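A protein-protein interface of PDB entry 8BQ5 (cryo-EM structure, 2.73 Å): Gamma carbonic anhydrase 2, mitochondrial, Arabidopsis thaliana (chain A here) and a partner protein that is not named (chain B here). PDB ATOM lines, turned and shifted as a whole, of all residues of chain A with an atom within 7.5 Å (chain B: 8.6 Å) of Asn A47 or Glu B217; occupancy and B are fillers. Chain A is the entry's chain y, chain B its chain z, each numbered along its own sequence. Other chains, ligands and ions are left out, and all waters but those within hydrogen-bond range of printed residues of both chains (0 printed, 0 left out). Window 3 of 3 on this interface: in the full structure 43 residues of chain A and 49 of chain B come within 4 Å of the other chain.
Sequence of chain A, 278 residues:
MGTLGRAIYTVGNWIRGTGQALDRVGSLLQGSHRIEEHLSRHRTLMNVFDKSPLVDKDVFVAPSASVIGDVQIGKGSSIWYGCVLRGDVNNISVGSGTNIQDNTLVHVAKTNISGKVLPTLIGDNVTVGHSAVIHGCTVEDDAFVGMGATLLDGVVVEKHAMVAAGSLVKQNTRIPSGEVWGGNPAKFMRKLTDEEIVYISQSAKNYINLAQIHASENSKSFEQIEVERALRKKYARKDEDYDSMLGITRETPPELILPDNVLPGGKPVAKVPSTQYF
O of Val A67 sits at hydrogen-bond distance from N of Met A46.
OD1 of Asn A47 sits at hydrogen-bond distance from OG of Ser A52, 2.6 Å away.
The side-chain hydroxyl (OH) of Tyr B81 lies within hydrogen-bond range of a ring nitrogen (ND1) of His B214, at 2.7 Å.
OH of Tyr B81 lies within hydrogen-bond range of ND2 of Asn B218 (3.3 Å).
The side-chain amide nitrogen (ND2) of Asn B218 sits at hydrogen-bond distance from the backbone carbonyl oxygen (O) of His B214 (2.9 Å).
The side-chain amino group of Lys B220 lies within salt-bridge range of the side-chain carboxylate of Glu B217, at 3.1 Å.
Of the printed residues of chain B, Phe A49 touches Leu B210 (3.6 Å) and Ala B213 (3.6 Å).
Pro A53 touches none of the printed residues of chain B.
Of the printed residues of chain A, Pro B63 touches Arg A41 (3.97 Å).
Glu B217 touches just one residue of chain A: Asn A47.
Printed residues of chain A within 4 Å of Ala B219: Arg A41.
Of the printed residues of chain A, Lys B220 touches Arg A41 and Arg A43.
Of the printed residues of chain A, Pro B221 touches Arg A43 (3.6 Å).
The nearest printed residue of chain A that does not touch Glu B217 is Met A46 (4.2 Å).
O of Asn B218 is in hydrogen-bond range of NH2 of Arg A41.
O of Lys B220 is in hydrogen-bond range of NH2 of Arg A41 (3.1 Å).
The backbone carbonyl oxygen of Asn B218 sits at hydrogen-bond distance from the guanidinium group of Arg A43 (2.8 Å).
NH2 of Arg A43 is in hydrogen-bond range of O of Lys B220 (2.7 Å).
The side-chain sulfur of Met A46 lies close to the side-chain amide oxygen of Asn B218, 3.2 Å away.
Among the printed residues, pairs that only touch across the chains: Arg A41 with Pro B63, Arg A41 with Ala B219, Arg A41 with Leu B222, Arg A43 with Pro B221, Met A46 with Tyr B81, Asn A47 with Glu B217, Phe A49 with Leu B210, Phe A49 with Ala B213, Ile A68 with Tyr B81 and Ile A68 with His B214.
Hydrophobic or aromatic side chains of chain B that line the printed part of chain A: Pro B63, Tyr B81, Leu B210, Ala B213, His B214 and Leu B222.
Of the 15 printed residues of chain A, 6 touch a printed residue of chain B.
Hydrophobic or aromatic side chains of chain A that line the printed part of chain B: Met A46, Phe A49 and Ile A68.
Along chain A the printed residues that touch a printed residue of chain B span positions 41 to 68.
Among the printed residues, 15 pairs touch across the chains.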
ATOM      1  N   ARG A  41     -32.291  21.334  -2.434  1.00  0.00           N
ATOM      2  CA  ARG A  41     -32.023  22.656  -1.806  1.00  0.00           C
ATOM      3  C   ARG A  41     -31.060  22.505  -0.623  1.00  0.00           C
ATOM      4  O   ARG A  41     -30.872  23.490   0.103  1.00  0.00           O
ATOM      5  CB  ARG A  41     -33.333  23.268  -1.316  1.00  0.00           C
ATOM      6  CG  ARG A  41     -34.251  23.740  -2.434  1.00  0.00           C
ATOM      7  CD  ARG A  41     -35.275  24.745  -1.950  1.00  0.00           C
ATOM      8  NE  ARG A  41     -34.663  25.992  -1.513  1.00  0.00           N
ATOM      9  CZ  ARG A  41     -34.484  27.061  -2.281  1.00  0.00           C
ATOM     10  NH1 ARG A  41     -34.878  27.046  -3.543  1.00  0.00           N
ATOM     11  NH2 ARG A  41     -33.915  28.144  -1.784  1.00  0.00           N
ATOM     12  N   ARG A  43     -27.691  22.709   1.289  1.00  0.00           N
ATOM     13  CA  ARG A  43     -26.412  23.436   1.104  1.00  0.00           C
ATOM     14  C   ARG A  43     -25.357  22.763   1.979  1.00  0.00           C
ATOM     15  O   ARG A  43     -25.539  22.742   3.203  1.00  0.00           O
ATOM     16  CB  ARG A  43     -26.568  24.923   1.437  1.00  0.00           C
ATOM     17  CG  ARG A  43     -27.444  25.686   0.454  1.00  0.00           C
ATOM     18  CD  ARG A  43     -28.107  26.876   1.118  1.00  0.00           C
ATOM     19  NE  ARG A  43     -28.413  27.954   0.191  1.00  0.00           N
ATOM     20  CZ  ARG A  43     -29.607  28.188  -0.337  1.00  0.00           C
ATOM     21  NH1 ARG A  43     -30.636  27.416  -0.033  1.00  0.00           N
ATOM     22  NH2 ARG A  43     -29.768  29.200  -1.168  1.00  0.00           N
ATOM     23  N   LEU A  45     -22.247  23.769   2.422  1.00  0.00           N
ATOM     24  CA  LEU A  45     -21.577  24.868   3.156  1.00  0.00           C
ATOM     25  C   LEU A  45     -22.519  26.063   3.134  1.00  0.00           C
ATOM     26  O   LEU A  45     -22.937  26.449   2.031  1.00  0.00           O
ATOM     27  CB  LEU A  45     -20.266  25.197   2.436  1.00  0.00           C
ATOM     28  CG  LEU A  45     -18.984  24.652   3.054  1.00  0.00           C
ATOM     29  CD1 LEU A  45     -18.808  23.179   2.724  1.00  0.00           C
ATOM     30  CD2 LEU A  45     -17.793  25.444   2.546  1.00  0.00           C
ATOM     31  N   MET A  46     -22.859  26.607   4.299  1.00  0.00           N
ATOM     32  CA  MET A  46     -23.860  27.699   4.334  1.00  0.00           C
ATOM     33  C   MET A  46     -23.450  28.792   5.318  1.00  0.00           C
ATOM     34  O   MET A  46     -22.965  28.452   6.401  1.00  0.00           O
ATOM     35  CB  MET A  46     -25.231  27.148   4.736  1.00  0.00           C
ATOM     36  CG  MET A  46     -26.386  28.029   4.321  1.00  0.00           C
ATOM     37  SD  MET A  46     -27.956  27.384   4.927  1.00  0.00           S
ATOM     38  CE  MET A  46     -27.967  28.046   6.592  1.00  0.00           C
ATOM     39  N   ASN A  47     -23.648  30.057   4.950  1.00  0.00           N
ATOM     40  CA  ASN A  47     -23.391  31.158   5.865  1.00  0.00           C
ATOM     41  C   ASN A  47     -24.570  31.338   6.807  1.00  0.00           C
ATOM     42  O   ASN A  47     -25.682  30.890   6.531  1.00  0.00           O
ATOM     43  CB  ASN A  47     -23.152  32.464   5.106  1.00  0.00           C
ATOM     44  CG  ASN A  47     -22.182  32.306   3.965  1.00  0.00           C
ATOM     45  OD1 ASN A  47     -20.971  32.301   4.162  1.00  0.00           O
ATOM     46  ND2 ASN A  47     -22.708  32.188   2.754  1.00  0.00           N
ATOM     47  N   VAL A  48     -24.312  31.992   7.934  1.00  0.00           N
ATOM     48  CA  VAL A  48     -25.375  32.445   8.823  1.00  0.00           C
ATOM     49  C   VAL A  48     -24.799  33.543   9.701  1.00  0.00           C
ATOM     50  O   VAL A  48     -23.641  33.477  10.121  1.00  0.00           O
ATOM     51  CB  VAL A  48     -25.973  31.278   9.649  1.00  0.00           C
ATOM     52  CG1 VAL A  48     -24.958  30.720  10.630  1.00  0.00           C
ATOM     53  CG2 VAL A  48     -27.235  31.726  10.368  1.00  0.00           C
ATOM     54  N   PHE A  49     -25.607  34.577   9.944  1.00  0.00           N
ATOM     55  CA  PHE A  49     -25.184  35.759  10.701  1.00  0.00           C
ATOM     56  C   PHE A  49     -23.896  36.352  10.134  1.00  0.00           C
ATOM     57  O   PHE A  49     -23.024  36.803  10.879  1.00  0.00           O
ATOM     58  CB  PHE A  49     -25.017  35.449  12.189  1.00  0.00           C
ATOM     59  CG  PHE A  49     -26.262  34.951  12.852  1.00  0.00           C
ATOM     60  CD1 PHE A  49     -27.439  35.677  12.783  1.00  0.00           C
ATOM     61  CD2 PHE A  49     -26.248  33.772  13.573  1.00  0.00           C
ATOM     62  CE1 PHE A  49     -28.583  35.222  13.406  1.00  0.00           C
ATOM     63  CE2 PHE A  49     -27.385  33.316  14.198  1.00  0.00           C
ATOM     64  CZ  PHE A  49     -28.555  34.040  14.114  1.00  0.00           C
ATOM     65  N   ASP A  50     -23.781  36.349   8.805  1.00  0.00           N
ATOM     66  CA  ASP A  50     -22.613  36.884   8.103  1.00  0.00           C
ATOM     67  C   ASP A  50     -21.318  36.208   8.551  1.00  0.00           C
ATOM     68  O   ASP A  50     -20.274  36.850   8.684  1.00  0.00           O
ATOM     69  CB  ASP A  50     -22.516  38.402   8.268  1.00  0.00           C
ATOM     70  CG  ASP A  50     -23.133  39.149   7.108  1.00  0.00           C
ATOM     71  OD1 ASP A  50     -22.565  39.093   5.997  1.00  0.00           O
ATOM     72  OD2 ASP A  50     -24.188  39.788   7.304  1.00  0.00           O
ATOM     73  N   LYS A  51     -21.385  34.901   8.784  1.00  0.00           N
ATOM     74  CA  LYS A  51     -20.223  34.090   9.121  1.00  0.00           C
ATOM     75  C   LYS A  51     -20.077  33.004   8.067  1.00  0.00           C
ATOM     76  O   LYS A  51     -21.047  32.304   7.759  1.00  0.00           O
ATOM     77  CB  LYS A  51     -20.363  33.470  10.515  1.00  0.00           C
ATOM     78  CG  LYS A  51     -20.179  34.452  11.665  1.00  0.00           C
ATOM     79  CD  LYS A  51     -18.729  34.888  11.814  1.00  0.00           C
ATOM     80  CE  LYS A  51     -18.627  36.243  12.499  1.00  0.00           C
ATOM     81  NZ  LYS A  51     -17.816  36.198  13.747  1.00  0.00           N
ATOM     82  N   SER A  52     -18.874  32.863   7.516  1.00  0.00           N
ATOM     83  CA  SER A  52     -18.632  31.934   6.424  1.00  0.00           C
ATOM     84  C   SER A  52     -17.681  30.831   6.855  1.00  0.00           C
ATOM     85  O   SER A  52     -16.605  31.129   7.392  1.00  0.00           O
ATOM     86  CB  SER A  52     -18.053  32.670   5.212  1.00  0.00           C
ATOM     87  OG  SER A  52     -18.370  31.997   4.008  1.00  0.00           O
ATOM     88  N   PRO A  53     -18.033  29.563   6.647  1.00  0.00           N
ATOM     89  CA  PRO A  53     -17.113  28.476   7.003  1.00  0.00           C
ATOM     90  C   PRO A  53     -15.809  28.562   6.223  1.00  0.00           C
ATOM     91  O   PRO A  53     -15.792  28.866   5.028  1.00  0.00           O
ATOM     92  CB  PRO A  53     -17.901  27.208   6.648  1.00  0.00           C
ATOM     93  CG  PRO A  53     -19.011  27.653   5.768  1.00  0.00           C
ATOM     94  CD  PRO A  53     -19.319  29.066   6.130  1.00  0.00           C
ATOM     95  N   VAL A  67     -22.299  22.012   6.976  1.00  0.00           N
ATOM     96  CA  VAL A  67     -21.318  22.871   7.628  1.00  0.00           C
ATOM     97  C   VAL A  67     -21.871  24.289   7.587  1.00  0.00           C
ATOM     98  O   VAL A  67     -21.974  24.894   6.513  1.00  0.00           O
ATOM     99  CB  VAL A  67     -19.944  22.781   6.953  1.00  0.00           C
ATOM    100  CG1 VAL A  67     -18.884  23.423   7.824  1.00  0.00           C
ATOM    101  CG2 VAL A  67     -19.595  21.330   6.671  1.00  0.00           C
ATOM    102  N   ILE A  68     -22.220  24.827   8.752  1.00  0.00           N
ATOM    103  CA  ILE A  68     -22.983  26.065   8.845  1.00  0.00           C
ATOM    104  C   ILE A  68     -22.241  27.053   9.733  1.00  0.00           C
ATOM    105  O   ILE A  68     -21.779  26.693  10.820  1.00  0.00           O
ATOM    106  CB  ILE A  68     -24.400  25.815   9.394  1.00  0.00           C
ATOM    107  CG1 ILE A  68     -25.202  24.950   8.423  1.00  0.00           C
ATOM    108  CG2 ILE A  68     -25.119  27.126   9.637  1.00  0.00           C
ATOM    109  CD1 ILE A  68     -26.196  24.053   9.101  1.00  0.00           C
ATOM    110  N   GLY A  69     -22.132  28.295   9.271  1.00  0.00           N
ATOM    111  CA  GLY A  69     -21.670  29.376  10.116  1.00  0.00           C
ATOM    112  C   GLY A  69     -20.171  29.472  10.294  1.00  0.00           C
ATOM    113  O   GLY A  69     -19.402  29.181   9.376  1.00  0.00           O
ATOM    114  N   ASP A  70     -19.747  29.884  11.488  1.00  0.00           N
ATOM    115  CA  ASP A  70     -18.343  30.186  11.761  1.00  0.00           C
ATOM    116  C   ASP A  70     -17.651  28.880  12.151  1.00  0.00           C
ATOM    117  O   ASP A  70     -17.524  28.518  13.322  1.00  0.00           O
ATOM    118  CB  ASP A  70     -18.247  31.271  12.832  1.00  0.00           C
ATOM    119  CG  ASP A  70     -16.922  31.281  13.563  1.00  0.00           C
ATOM    120  OD1 ASP A  70     -15.870  31.056  12.929  1.00  0.00           O
ATOM    121  OD2 ASP A  70     -16.937  31.539  14.782  1.00  0.00           O
ATOM    122  N   PHE B  60     -40.053  26.410  10.760  1.00  0.00           N
ATOM    123  CA  PHE B  60     -38.886  26.148   9.931  1.00  0.00           C
ATOM    124  C   PHE B  60     -38.624  24.651   9.860  1.00  0.00           C
ATOM    125  O   PHE B  60     -38.626  23.960  10.883  1.00  0.00           O
ATOM    126  CB  PHE B  60     -37.657  26.874  10.482  1.00  0.00           C
ATOM    127  CG  PHE B  60     -36.354  26.416   9.879  1.00  0.00           C
ATOM    128  CD1 PHE B  60     -36.169  26.395   8.508  1.00  0.00           C
ATOM    129  CD2 PHE B  60     -35.312  26.011  10.687  1.00  0.00           C
ATOM    130  CE1 PHE B  60     -34.970  25.974   7.962  1.00  0.00           C
ATOM    131  CE2 PHE B  60     -34.115  25.582  10.147  1.00  0.00           C
ATOM    132  CZ  PHE B  60     -33.944  25.567   8.784  1.00  0.00           C
ATOM    133  N   PRO B  63     -34.022  21.670   4.951  1.00  0.00           N
ATOM    134  CA  PRO B  63     -34.244  20.931   3.697  1.00  0.00           C
ATOM    135  C   PRO B  63     -33.849  19.466   3.773  1.00  0.00           C
ATOM    136  O   PRO B  63     -34.457  18.633   3.092  1.00  0.00           O
ATOM    137  CB  PRO B  63     -33.392  21.705   2.681  1.00  0.00           C
ATOM    138  CG  PRO B  63     -33.243  23.064   3.264  1.00  0.00           C
ATOM    139  CD  PRO B  63     -33.208  22.880   4.750  1.00  0.00           C
ATOM    140  N   TYR B  81     -31.574  20.211  11.137  1.00  0.00           N
ATOM    141  CA  TYR B  81     -30.906  19.432  10.102  1.00  0.00           C
ATOM    142  C   TYR B  81     -30.794  17.963  10.490  1.00  0.00           C
ATOM    143  O   TYR B  81     -30.418  17.633  11.618  1.00  0.00           O
ATOM    144  CB  TYR B  81     -29.523  20.021   9.836  1.00  0.00           C
ATOM    145  CG  TYR B  81     -29.581  21.485   9.473  1.00  0.00           C
ATOM    146  CD1 TYR B  81     -29.780  21.888   8.161  1.00  0.00           C
ATOM    147  CD2 TYR B  81     -29.476  22.464  10.452  1.00  0.00           C
ATOM    148  CE1 TYR B  81     -29.848  23.225   7.831  1.00  0.00           C
ATOM    149  CE2 TYR B  81     -29.548  23.800  10.132  1.00  0.00           C
ATOM    150  CZ  TYR B  81     -29.732  24.177   8.822  1.00  0.00           C
ATOM    151  OH  TYR B  81     -29.800  25.510   8.503  1.00  0.00           O
ATOM    152  N   LEU B 210     -33.587  31.737  16.455  1.00  0.00           N
ATOM    153  CA  LEU B 210     -32.475  31.164  15.647  1.00  0.00           C
ATOM    154  C   LEU B 210     -33.066  30.475  14.414  1.00  0.00           C
ATOM    155  O   LEU B 210     -32.495  30.634  13.331  1.00  0.00           O
ATOM    156  CB  LEU B 210     -31.711  30.166  16.522  1.00  0.00           C
ATOM    157  CG  LEU B 210     -30.401  29.625  15.955  1.00  0.00           C
ATOM    158  CD1 LEU B 210     -29.421  30.756  15.693  1.00  0.00           C
ATOM    159  CD2 LEU B 210     -29.791  28.610  16.910  1.00  0.00           C
ATOM    160  N   ALA B 211     -34.157  29.727  14.586  1.00  0.00           N
ATOM    161  CA  ALA B 211     -34.832  29.060  13.453  1.00  0.00           C
ATOM    162  C   ALA B 211     -35.266  30.114  12.445  1.00  0.00           C
ATOM    163  O   ALA B 211     -35.090  29.869  11.253  1.00  0.00           O
ATOM    164  CB  ALA B 211     -36.028  28.279  13.929  1.00  0.00           C
ATOM    165  N   GLN B 212     -35.823  31.230  12.919  1.00  0.00           N
ATOM    166  CA  GLN B 212     -36.174  32.283  11.967  1.00  0.00           C
ATOM    167  C   GLN B 212     -34.959  32.696  11.144  1.00  0.00           C
ATOM    168  O   GLN B 212     -35.043  32.854   9.918  1.00  0.00           O
ATOM    169  CB  GLN B 212     -36.761  33.488  12.702  1.00  0.00           C
ATOM    170  CG  GLN B 212     -38.276  33.462  12.882  1.00  0.00           C
ATOM    171  CD  GLN B 212     -39.000  32.611  11.852  1.00  0.00           C
ATOM    172  OE1 GLN B 212     -38.843  32.796  10.643  1.00  0.00           O
ATOM    173  NE2 GLN B 212     -39.802  31.668  12.332  1.00  0.00           N
ATOM    174  N   ALA B 213     -33.811  32.857  11.807  1.00  0.00           N
ATOM    175  CA  ALA B 213     -32.595  33.213  11.078  1.00  0.00           C
ATOM    176  C   ALA B 213     -32.225  32.146  10.050  1.00  0.00           C
ATOM    177  O   ALA B 213     -31.925  32.463   8.891  1.00  0.00           O
ATOM    178  CB  ALA B 213     -31.439  33.442  12.050  1.00  0.00           C
ATOM    179  N   HIS B 214     -32.258  30.872  10.449  1.00  0.00           N
ATOM    180  CA  HIS B 214     -31.889  29.801   9.525  1.00  0.00           C
ATOM    181  C   HIS B 214     -32.890  29.656   8.385  1.00  0.00           C
ATOM    182  O   HIS B 214     -32.493  29.370   7.251  1.00  0.00           O
ATOM    183  CB  HIS B 214     -31.749  28.476  10.270  1.00  0.00           C
ATOM    184  CG  HIS B 214     -30.397  28.265  10.874  1.00  0.00           C
ATOM    185  ND1 HIS B 214     -29.465  27.406  10.332  1.00  0.00           N
ATOM    186  CD2 HIS B 214     -29.822  28.795  11.978  1.00  0.00           C
ATOM    187  CE1 HIS B 214     -28.373  27.420  11.073  1.00  0.00           C
ATOM    188  NE2 HIS B 214     -28.564  28.254  12.080  1.00  0.00           N
ATOM    189  N   ALA B 215     -34.183  29.824   8.668  1.00  0.00           N
ATOM    190  CA  ALA B 215     -35.196  29.742   7.623  1.00  0.00           C
ATOM    191  C   ALA B 215     -35.018  30.854   6.604  1.00  0.00           C
ATOM    192  O   ALA B 215     -35.169  30.630   5.398  1.00  0.00           O
ATOM    193  CB  ALA B 215     -36.594  29.797   8.236  1.00  0.00           C
ATOM    194  N   ALA B 216     -34.493  32.000   7.024  1.00  0.00           N
ATOM    195  CA  ALA B 216     -34.224  33.081   6.042  1.00  0.00           C
ATOM    196  C   ALA B 216     -33.049  32.741   5.108  1.00  0.00           C
ATOM    197  O   ALA B 216     -33.224  32.899   3.886  1.00  0.00           O
ATOM    198  CB  ALA B 216     -34.026  34.391   6.759  1.00  0.00           C
ATOM    199  N   GLU B 217     -31.904  32.299   5.631  1.00  0.00           N
ATOM    200  CA  GLU B 217     -30.697  32.057   4.778  1.00  0.00           C
ATOM    201  C   GLU B 217     -30.924  30.891   3.800  1.00  0.00           C
ATOM    202  O   GLU B 217     -30.323  30.926   2.713  1.00  0.00           O
ATOM    203  CB  GLU B 217     -29.456  31.811   5.637  1.00  0.00           C
ATOM    204  CG  GLU B 217     -28.156  32.066   4.902  1.00  0.00           C
ATOM    205  CD  GLU B 217     -27.586  33.465   5.056  1.00  0.00           C
ATOM    206  OE1 GLU B 217     -27.981  34.161   6.012  1.00  0.00           O
ATOM    207  OE2 GLU B 217     -26.742  33.852   4.223  1.00  0.00           O
ATOM    208  N   ASN B 218     -31.719  29.891   4.176  1.00  0.00           N
ATOM    209  CA  ASN B 218     -32.038  28.750   3.278  1.00  0.00           C
ATOM    210  C   ASN B 218     -32.972  29.226   2.156  1.00  0.00           C
ATOM    211  O   ASN B 218     -32.907  28.646   1.064  1.00  0.00           O
ATOM    212  CB  ASN B 218     -32.635  27.565   4.049  1.00  0.00           C
ATOM    213  CG  ASN B 218     -31.607  26.749   4.802  1.00  0.00           C
ATOM    214  OD1 ASN B 218     -30.810  26.039   4.197  1.00  0.00           O
ATOM    215  ND2 ASN B 218     -31.633  26.819   6.122  1.00  0.00           N
ATOM    216  N   ALA B 219     -33.805  30.235   2.418  1.00  0.00           N
ATOM    217  CA  ALA B 219     -34.753  30.776   1.411  1.00  0.00           C
ATOM    218  C   ALA B 219     -34.007  31.491   0.276  1.00  0.00           C
ATOM    219  O   ALA B 219     -34.598  31.632  -0.808  1.00  0.00           O
ATOM    220  CB  ALA B 219     -35.713  31.708   2.088  1.00  0.00           C
ATOM    221  N   LYS B 220     -32.775  31.930   0.519  1.00  0.00           N
ATOM    222  CA  LYS B 220     -31.961  32.625  -0.512  1.00  0.00           C
ATOM    223  C   LYS B 220     -32.051  31.864  -1.837  1.00  0.00           C
ATOM    224  O   LYS B 220     -32.012  30.619  -1.818  1.00  0.00           O
ATOM    225  CB  LYS B 220     -30.500  32.730  -0.068  1.00  0.00           C
ATOM    226  CG  LYS B 220     -30.050  34.090   0.440  1.00  0.00           C
ATOM    227  CD  LYS B 220     -30.538  34.406   1.831  1.00  0.00           C
ATOM    228  CE  LYS B 220     -29.944  35.684   2.382  1.00  0.00           C
ATOM    229  NZ  LYS B 220     -28.462  35.664   2.332  1.00  0.00           N
ATOM    230  N   PRO B 221     -32.188  32.553  -2.987  1.00  0.00           N
ATOM    231  CA  PRO B 221     -32.211  31.885  -4.284  1.00  0.00           C
ATOM    232  C   PRO B 221     -30.962  31.015  -4.467  1.00  0.00           C
ATOM    233  O   PRO B 221     -29.889  31.428  -4.055  1.00  0.00           O
ATOM    234  CB  PRO B 221     -32.219  33.025  -5.317  1.00  0.00           C
ATOM    235  CG  PRO B 221     -31.844  34.264  -4.529  1.00  0.00           C
ATOM    236  CD  PRO B 221     -32.315  34.005  -3.113  1.00  0.00           C
ATOM    237  N   LEU B 222     -31.134  29.844  -5.081  1.00  0.00           N
ATOM    238  CA  LEU B 222     -29.987  28.939  -5.356  1.00  0.00           C
ATOM    239  C   LEU B 222     -28.968  29.665  -6.237  1.00  0.00           C
ATOM    240  O   LEU B 222     -29.376  30.208  -7.277  1.00  0.00           O
ATOM    241  CB  LEU B 222     -30.532  27.688  -6.045  1.00  0.00           C
ATOM    242  CG  LEU B 222     -31.665  26.990  -5.297  1.00  0.00           C
ATOM    243  CD1 LEU B 222     -32.369  25.982  -6.192  1.00  0.00           C
ATOM    244  CD2 LEU B 222     -31.150  26.327  -4.030  1.00  0.00           C
ATOM    245  N   GLU B 226     -22.674  28.492  -8.530  1.00  0.00           N
ATOM    246  CA  GLU B 226     -22.338  27.124  -8.140  1.00  0.00           C
ATOM    247  C   GLU B 226     -22.908  26.111  -9.125  1.00  0.00           C
ATOM    248  O   GLU B 226     -22.271  25.091  -9.422  1.00  0.00           O
ATOM    249  CB  GLU B 226     -22.845  26.836  -6.727  1.00  0.00           C
ATOM    250  CG  GLU B 226     -22.376  27.832  -5.689  1.00  0.00           C
ATOM    251  CD  GLU B 226     -21.165  27.342  -4.927  1.00  0.00           C
ATOM    252  OE1 GLU B 226     -20.987  26.110  -4.821  1.00  0.00           O
ATOM    253  OE2 GLU B 226     -20.385  28.186  -4.439  1.00  0.00           O
